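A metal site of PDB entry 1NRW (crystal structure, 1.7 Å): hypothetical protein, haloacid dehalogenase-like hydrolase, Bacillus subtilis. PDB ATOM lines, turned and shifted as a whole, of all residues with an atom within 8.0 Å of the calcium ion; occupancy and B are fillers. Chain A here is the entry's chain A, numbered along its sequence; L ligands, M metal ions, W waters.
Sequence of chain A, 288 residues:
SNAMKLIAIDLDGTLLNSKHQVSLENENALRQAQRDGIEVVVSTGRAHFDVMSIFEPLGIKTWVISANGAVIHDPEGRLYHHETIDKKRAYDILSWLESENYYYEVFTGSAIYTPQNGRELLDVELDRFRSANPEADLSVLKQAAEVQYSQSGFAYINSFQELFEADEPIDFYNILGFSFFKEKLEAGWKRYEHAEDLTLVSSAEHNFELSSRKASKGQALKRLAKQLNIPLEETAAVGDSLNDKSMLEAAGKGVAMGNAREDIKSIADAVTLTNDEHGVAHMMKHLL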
ATOM      1  N   ASP A  10     -20.570  18.628   9.652  1.00  0.00           N
ATOM      2  CA  ASP A  10     -20.012  19.207   8.427  1.00  0.00           C
ATOM      3  C   ASP A  10     -20.000  20.723   8.584  1.00  0.00           C
ATOM      4  O   ASP A  10     -20.799  21.285   9.339  1.00  0.00           O
ATOM      5  CB  ASP A  10     -20.878  18.778   7.241  1.00  0.00           C
ATOM      6  CG  ASP A  10     -20.328  19.232   5.909  1.00  0.00           C
ATOM      7  OD1 ASP A  10     -19.137  19.602   5.797  1.00  0.00           O
ATOM      8  OD2 ASP A  10     -21.112  19.199   4.948  1.00  0.00           O
ATOM      9  N   LEU A  11     -19.075  21.392   7.891  1.00  0.00           N
ATOM     10  CA  LEU A  11     -18.956  22.853   8.003  1.00  0.00           C
ATOM     11  C   LEU A  11     -19.882  23.578   7.032  1.00  0.00           C
ATOM     12  O   LEU A  11     -20.934  24.073   7.425  1.00  0.00           O
ATOM     13  CB  LEU A  11     -17.498  23.257   7.768  1.00  0.00           C
ATOM     14  CG  LEU A  11     -17.154  24.752   7.883  1.00  0.00           C
ATOM     15  CD1 LEU A  11     -17.237  25.237   9.327  1.00  0.00           C
ATOM     16  CD2 LEU A  11     -15.751  24.948   7.330  1.00  0.00           C
ATOM     17  N   ASP A  12     -19.485  23.648   5.759  1.00  0.00           N
ATOM     18  CA  ASP A  12     -20.304  24.330   4.752  1.00  0.00           C
ATOM     19  C   ASP A  12     -21.684  23.677   4.595  1.00  0.00           C
ATOM     20  O   ASP A  12     -21.802  22.461   4.664  1.00  0.00           O
ATOM     21  CB  ASP A  12     -19.592  24.314   3.402  1.00  0.00           C
ATOM     22  CG  ASP A  12     -18.352  25.189   3.391  1.00  0.00           C
ATOM     23  OD1 ASP A  12     -18.492  26.405   3.174  1.00  0.00           O
ATOM     24  OD2 ASP A  12     -17.243  24.659   3.628  1.00  0.00           O
ATOM     25  N   GLY A  13     -22.715  24.490   4.403  1.00  0.00           N
ATOM     26  CA  GLY A  13     -24.060  23.971   4.202  1.00  0.00           C
ATOM     27  C   GLY A  13     -24.676  23.216   5.360  1.00  0.00           C
ATOM     28  O   GLY A  13     -25.795  22.702   5.259  1.00  0.00           O
ATOM     29  N   THR A  14     -23.956  23.152   6.478  1.00  0.00           N
ATOM     30  CA  THR A  14     -24.421  22.418   7.648  1.00  0.00           C
ATOM     31  C   THR A  14     -24.300  23.314   8.875  1.00  0.00           C
ATOM     32  O   THR A  14     -25.290  23.928   9.293  1.00  0.00           O
ATOM     33  CB  THR A  14     -23.609  21.108   7.780  1.00  0.00           C
ATOM     34  OG1 THR A  14     -23.859  20.302   6.621  1.00  0.00           O
ATOM     35  CG2 THR A  14     -24.009  20.317   9.021  1.00  0.00           C
ATOM     36  N   LEU A  15     -23.109  23.398   9.459  1.00  0.00           N
ATOM     37  CA  LEU A  15     -22.917  24.260  10.621  1.00  0.00           C
ATOM     38  C   LEU A  15     -23.056  25.722  10.185  1.00  0.00           C
ATOM     39  O   LEU A  15     -23.629  26.555  10.900  1.00  0.00           O
ATOM     40  CB  LEU A  15     -21.535  24.063  11.247  1.00  0.00           C
ATOM     41  CG  LEU A  15     -21.246  24.927  12.487  1.00  0.00           C
ATOM     42  CD1 LEU A  15     -22.186  24.508  13.623  1.00  0.00           C
ATOM     43  CD2 LEU A  15     -19.796  24.760  12.916  1.00  0.00           C
ATOM     44  N   LEU A  16     -22.530  26.025   9.004  1.00  0.00           N
ATOM     45  CA  LEU A  16     -22.608  27.391   8.490  1.00  0.00           C
ATOM     46  C   LEU A  16     -23.915  27.649   7.745  1.00  0.00           C
ATOM     47  O   LEU A  16     -24.402  26.765   7.027  1.00  0.00           O
ATOM     48  CB  LEU A  16     -21.454  27.666   7.534  1.00  0.00           C
ATOM     49  CG  LEU A  16     -20.046  27.504   8.140  1.00  0.00           C
ATOM     50  CD1 LEU A  16     -19.004  27.721   7.060  1.00  0.00           C
ATOM     51  CD2 LEU A  16     -19.842  28.493   9.275  1.00  0.00           C
ATOM     52  N   SER A  43     -16.102  18.581  10.537  1.00  0.00           N
ATOM     53  CA  SER A  43     -15.433  17.930   9.403  1.00  0.00           C
ATOM     54  C   SER A  43     -15.643  18.645   8.076  1.00  0.00           C
ATOM     55  O   SER A  43     -16.775  18.870   7.653  1.00  0.00           O
ATOM     56  CB  SER A  43     -15.949  16.490   9.301  1.00  0.00           C
ATOM     57  OG  SER A  43     -15.237  15.772   8.307  1.00  0.00           O
ATOM     58  N   THR A  44     -14.547  18.960   7.402  1.00  0.00           N
ATOM     59  CA  THR A  44     -14.607  19.716   6.158  1.00  0.00           C
ATOM     60  C   THR A  44     -13.564  19.320   5.114  1.00  0.00           C
ATOM     61  O   THR A  44     -12.557  18.677   5.431  1.00  0.00           O
ATOM     62  CB  THR A  44     -14.428  21.226   6.457  1.00  0.00           C
ATOM     63  OG1 THR A  44     -14.545  21.991   5.252  1.00  0.00           O
ATOM     64  CG2 THR A  44     -13.038  21.481   7.062  1.00  0.00           C
ATOM     65  N   GLY A  45     -13.806  19.715   3.868  1.00  0.00           N
ATOM     66  CA  GLY A  45     -12.862  19.455   2.798  1.00  0.00           C
ATOM     67  C   GLY A  45     -11.867  20.607   2.757  1.00  0.00           C
ATOM     68  O   GLY A  45     -10.859  20.542   2.060  1.00  0.00           O
ATOM     69  N   ARG A 128     -19.794  26.645  -4.177  1.00  0.00           N
ATOM     70  CA  ARG A 128     -20.001  25.966  -2.897  1.00  0.00           C
ATOM     71  C   ARG A 128     -21.279  26.510  -2.253  1.00  0.00           C
ATOM     72  O   ARG A 128     -22.141  25.741  -1.823  1.00  0.00           O
ATOM     73  CB  ARG A 128     -18.838  26.211  -1.941  1.00  0.00           C
ATOM     74  CG  ARG A 128     -17.508  25.560  -2.284  1.00  0.00           C
ATOM     75  CD  ARG A 128     -16.491  26.040  -1.243  1.00  0.00           C
ATOM     76  NE  ARG A 128     -15.137  25.522  -1.396  1.00  0.00           N
ATOM     77  CZ  ARG A 128     -14.721  24.334  -0.951  1.00  0.00           C
ATOM     78  NH1 ARG A 128     -15.570  23.519  -0.327  1.00  0.00           N
ATOM     79  NH2 ARG A 128     -13.456  23.989  -1.071  1.00  0.00           N
ATOM     80  N   SER A 131     -24.499  25.581  -4.249  1.00  0.00           N
ATOM     81  CA  SER A 131     -24.824  24.164  -4.218  1.00  0.00           C
ATOM     82  C   SER A 131     -25.463  23.787  -2.882  1.00  0.00           C
ATOM     83  O   SER A 131     -26.360  22.952  -2.837  1.00  0.00           O
ATOM     84  CB  SER A 131     -23.556  23.330  -4.443  1.00  0.00           C
ATOM     85  OG  SER A 131     -23.052  23.559  -5.751  1.00  0.00           O
ATOM     86  N   ALA A 132     -24.992  24.414  -1.812  1.00  0.00           N
ATOM     87  CA  ALA A 132     -25.505  24.140  -0.469  1.00  0.00           C
ATOM     88  C   ALA A 132     -26.901  24.726  -0.282  1.00  0.00           C
ATOM     89  O   ALA A 132     -27.760  24.113   0.342  1.00  0.00           O
ATOM     90  CB  ALA A 132     -24.565  24.708   0.577  1.00  0.00           C
ATOM     91  N   SER A 202     -17.183  14.959  -3.946  1.00  0.00           N
ATOM     92  CA  SER A 202     -17.529  16.285  -4.450  1.00  0.00           C
ATOM     93  C   SER A 202     -18.154  17.056  -3.305  1.00  0.00           C
ATOM     94  O   SER A 202     -18.856  16.480  -2.464  1.00  0.00           O
ATOM     95  CB  SER A 202     -18.525  16.182  -5.613  1.00  0.00           C
ATOM     96  OG  SER A 202     -19.011  17.467  -5.981  1.00  0.00           O
ATOM     97  N   SER A 203     -17.902  18.370  -3.242  1.00  0.00           N
ATOM     98  CA  SER A 203     -18.453  19.213  -2.196  1.00  0.00           C
ATOM     99  C   SER A 203     -19.324  20.326  -2.792  1.00  0.00           C
ATOM    100  O   SER A 203     -19.829  21.176  -2.057  1.00  0.00           O
ATOM    101  CB  SER A 203     -17.341  19.832  -1.353  1.00  0.00           C
ATOM    102  OG  SER A 203     -16.523  20.691  -2.132  1.00  0.00           O
ATOM    103  N   ALA A 204     -19.473  20.310  -4.107  1.00  0.00           N
ATOM    104  CA  ALA A 204     -20.267  21.300  -4.825  1.00  0.00           C
ATOM    105  C   ALA A 204     -20.544  20.815  -6.250  1.00  0.00           C
ATOM    106  O   ALA A 204     -19.786  20.010  -6.793  1.00  0.00           O
ATOM    107  CB  ALA A 204     -19.549  22.648  -4.850  1.00  0.00           C
ATOM    108  N   LYS A 217     -14.054  11.579   5.088  1.00  0.00           N
ATOM    109  CA  LYS A 217     -14.652  12.037   6.334  1.00  0.00           C
ATOM    110  C   LYS A 217     -15.067  10.856   7.208  1.00  0.00           C
ATOM    111  O   LYS A 217     -14.919  10.900   8.426  1.00  0.00           O
ATOM    112  CB  LYS A 217     -15.856  12.953   6.057  1.00  0.00           C
ATOM    113  CG  LYS A 217     -15.442  14.291   5.458  1.00  0.00           C
ATOM    114  CD  LYS A 217     -16.614  15.276   5.423  1.00  0.00           C
ATOM    115  CE  LYS A 217     -16.198  16.612   4.814  1.00  0.00           C
ATOM    116  NZ  LYS A 217     -17.316  17.594   4.870  1.00  0.00           N
ATOM    117  N   VAL A 238     -23.691  14.618  10.815  1.00  0.00           N
ATOM    118  CA  VAL A 238     -24.686  15.388  10.072  1.00  0.00           C
ATOM    119  C   VAL A 238     -24.031  16.152   8.930  1.00  0.00           C
ATOM    120  O   VAL A 238     -22.920  16.661   9.071  1.00  0.00           O
ATOM    121  CB  VAL A 238     -25.428  16.376  11.033  1.00  0.00           C
ATOM    122  CG1 VAL A 238     -24.436  17.344  11.683  1.00  0.00           C
ATOM    123  CG2 VAL A 238     -26.507  17.123  10.299  1.00  0.00           C
ATOM    124  N   GLY A 239     -24.706  16.198   7.781  1.00  0.00           N
ATOM    125  CA  GLY A 239     -24.153  16.897   6.621  1.00  0.00           C
ATOM    126  C   GLY A 239     -25.186  17.109   5.530  1.00  0.00           C
ATOM    127  O   GLY A 239     -26.298  16.588   5.616  1.00  0.00           O
ATOM    128  N   ASP A 240     -24.815  17.847   4.486  1.00  0.00           N
ATOM    129  CA  ASP A 240     -25.716  18.136   3.366  1.00  0.00           C
ATOM    130  C   ASP A 240     -25.168  17.719   2.014  1.00  0.00           C
ATOM    131  O   ASP A 240     -25.920  17.456   1.091  1.00  0.00           O
ATOM    132  CB  ASP A 240     -25.998  19.644   3.289  1.00  0.00           C
ATOM    133  CG  ASP A 240     -24.759  20.442   2.919  1.00  0.00           C
ATOM    134  OD1 ASP A 240     -23.731  20.237   3.588  1.00  0.00           O
ATOM    135  OD2 ASP A 240     -24.787  21.263   1.968  1.00  0.00           O
ATOM    136  N   SER A 241     -23.838  17.664   1.904  1.00  0.00           N
ATOM    137  CA  SER A 241     -23.187  17.360   0.636  1.00  0.00           C
ATOM    138  C   SER A 241     -22.652  15.946   0.416  1.00  0.00           C
ATOM    139  O   SER A 241     -22.484  15.161   1.335  1.00  0.00           O
ATOM    140  CB  SER A 241     -22.084  18.390   0.415  1.00  0.00           C
ATOM    141  OG  SER A 241     -21.325  18.534   1.603  1.00  0.00           O
ATOM    142  N   LEU A 242     -22.347  15.649  -0.852  1.00  0.00           N
ATOM    143  CA  LEU A 242     -21.879  14.330  -1.240  1.00  0.00           C
ATOM    144  C   LEU A 242     -20.636  13.845  -0.494  1.00  0.00           C
ATOM    145  O   LEU A 242     -20.523  12.647  -0.234  1.00  0.00           O
ATOM    146  CB  LEU A 242     -21.627  14.288  -2.758  1.00  0.00           C
ATOM    147  CG  LEU A 242     -21.290  12.915  -3.335  1.00  0.00           C
ATOM    148  CD1 LEU A 242     -22.393  11.922  -2.987  1.00  0.00           C
ATOM    149  CD2 LEU A 242     -21.121  13.031  -4.850  1.00  0.00           C
ATOM    150  N   ASN A 243     -19.722  14.749  -0.156  1.00  0.00           N
ATOM    151  CA  ASN A 243     -18.510  14.353   0.561  1.00  0.00           C
ATOM    152  C   ASN A 243     -18.783  13.922   1.999  1.00  0.00           C
ATOM    153  O   ASN A 243     -17.876  13.477   2.701  1.00  0.00           O
ATOM    154  CB  ASN A 243     -17.473  15.491   0.509  1.00  0.00           C
ATOM    155  CG  ASN A 243     -17.999  16.800   1.103  1.00  0.00           C
ATOM    156  OD1 ASN A 243     -19.190  17.080   1.072  1.00  0.00           O
ATOM    157  ND2 ASN A 243     -17.076  17.607   1.641  1.00  0.00           N
ATOM    158  N   ASP A 244     -20.036  14.054   2.439  1.00  0.00           N
ATOM    159  CA  ASP A 244     -20.405  13.659   3.794  1.00  0.00           C
ATOM    160  C   ASP A 244     -20.968  12.243   3.845  1.00  0.00           C
ATOM    161  O   ASP A 244     -21.144  11.677   4.930  1.00  0.00           O
ATOM    162  CB  ASP A 244     -21.478  14.594   4.377  1.00  0.00           C
ATOM    163  CG  ASP A 244     -21.009  16.022   4.513  1.00  0.00           C
ATOM    164  OD1 ASP A 244     -19.808  16.229   4.795  1.00  0.00           O
ATOM    165  OD2 ASP A 244     -21.847  16.935   4.351  1.00  0.00           O
ATOM    166  N   MET A 247     -19.258   9.641   6.109  1.00  0.00           N
ATOM    167  CA  MET A 247     -19.331   9.773   7.563  1.00  0.00           C
ATOM    168  C   MET A 247     -20.727   9.473   8.101  1.00  0.00           C
ATOM    169  O   MET A 247     -20.863   9.000   9.220  1.00  0.00           O
ATOM    170  CB  MET A 247     -18.804  11.137   8.036  1.00  0.00           C
ATOM    171  CG  MET A 247     -19.720  12.317   7.935  1.00  0.00           C
ATOM    172  SD  MET A 247     -18.855  13.807   8.879  1.00  0.00           S
ATOM    173  CE  MET A 247     -19.884  15.228   8.069  1.00  0.00           C
ATOM    174  N   MET A 257     -29.128  17.261   6.494  1.00  0.00           N
ATOM    175  CA  MET A 257     -29.609  18.628   6.689  1.00  0.00           C
ATOM    176  C   MET A 257     -30.857  18.804   5.822  1.00  0.00           C
ATOM    177  O   MET A 257     -31.055  18.077   4.846  1.00  0.00           O
ATOM    178  CB  MET A 257     -28.538  19.631   6.241  1.00  0.00           C
ATOM    179  CG  MET A 257     -27.292  19.627   7.114  1.00  0.00           C
ATOM    180  SD  MET A 257     -27.703  20.173   8.923  1.00  0.00           S
ATOM    181  CE  MET A 257     -28.423  21.927   8.529  1.00  0.00           C
ATOM    182  N   ASN A 259     -31.462  21.063   3.758  1.00  0.00           N
ATOM    183  CA  ASN A 259     -31.035  21.518   2.436  1.00  0.00           C
ATOM    184  C   ASN A 259     -30.093  20.511   1.768  1.00  0.00           C
ATOM    185  O   ASN A 259     -29.447  20.829   0.770  1.00  0.00           O
ATOM    186  CB  ASN A 259     -30.305  22.864   2.567  1.00  0.00           C
ATOM    187  CG  ASN A 259     -29.193  22.831   3.605  1.00  0.00           C
ATOM    188  OD1 ASN A 259     -29.440  22.608   4.793  1.00  0.00           O
ATOM    189  ND2 ASN A 259     -27.952  23.044   3.165  1.00  0.00           N
ATOM    190  N   ARG A 261     -28.527  17.198  -0.268  1.00  0.00           N
ATOM    191  CA  ARG A 261     -28.718  16.600  -1.580  1.00  0.00           C
ATOM    192  C   ARG A 261     -29.663  15.425  -1.373  1.00  0.00           C
ATOM    193  O   ARG A 261     -29.708  14.850  -0.285  1.00  0.00           O
ATOM    194  CB  ARG A 261     -27.396  16.065  -2.125  1.00  0.00           C
ATOM    195  CG  ARG A 261     -26.381  17.129  -2.530  1.00  0.00           C
ATOM    196  CD  ARG A 261     -24.998  16.501  -2.652  1.00  0.00           C
ATOM    197  NE  ARG A 261     -24.987  15.285  -3.462  1.00  0.00           N
ATOM    198  CZ  ARG A 261     -24.992  15.266  -4.792  1.00  0.00           C
ATOM    199  NH1 ARG A 261     -25.000  16.403  -5.477  1.00  0.00           N
ATOM    200  NH2 ARG A 261     -24.967  14.099  -5.443  1.00  0.00           N
HETATM  201  P1  LIG L   1     -17.449  21.142   3.280  1.00  0.00           P
HETATM  202  O1  LIG L   1     -18.863  20.784   3.505  1.00  0.00           O
HETATM  203  O2  LIG L   1     -16.611  19.921   3.404  1.00  0.00           O
HETATM  204  O3  LIG L   1     -17.314  21.705   1.912  1.00  0.00           O
HETATM  205  O4  LIG L   1     -17.029  22.139   4.288  1.00  0.00           O
HETATM  206 CA    CA M   1     -21.335  20.626   3.006  1.00  0.00          CA
HETATM  207  O   HOH W   1     -22.244  22.195   1.294  1.00  0.00           O
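Merely in contact with the calcium ion: Asp 244. Of the 28 residues printed, 5 come within 4 Å of the calcium ion.
O of Asp 10 lies within hydrogen-bond range of N of Leu 15. The side-chain carboxylate (OD2) of Asp 10 lies close to the side-chain hydroxyl (OG1) of Thr 14, 3.4 Å away. The backbone carbonyl oxygen (O) of Asp 240 sits at hydrogen-bond distance from the backbone NH (N) of Arg 261, at 3.0 Å. O of Val 238 sits at hydrogen-bond distance from N of Asp 10, 3.1 Å away. The side-chain amide oxygen (OD1) of Asn 243 lies close to the side-chain hydroxyl (OG) of Ser 241 (2.6 Å). N of Ser 241 sits at hydrogen-bond distance from OD2 of Asp 244 (3.2 Å). The backbone NH (N) of Asp 240 is in hydrogen-bond range of the side-chain hydroxyl (OG1) of Thr 14, 3.4 Å away. The backbone NH of Asp 240 is in hydrogen-bond range of the side-chain carboxylate of Asp 244.
OD2 of Asp 10 is bound to the calcium ion (2.4 Å). The calcium ion is bound by water W1, 2.5 Å away. OD1 of Asp 240 binds the calcium ion, 2.5 Å away. The backbone carbonyl oxygen (O) of Asp 12 binds the calcium ion, at 2.5 Å. The calcium ion is bound by OG of Ser 241 (2.5 Å). O1 of the ligand is bound to the calcium ion (2.5 Å). The calcium ion has six donor atoms within binding distance.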
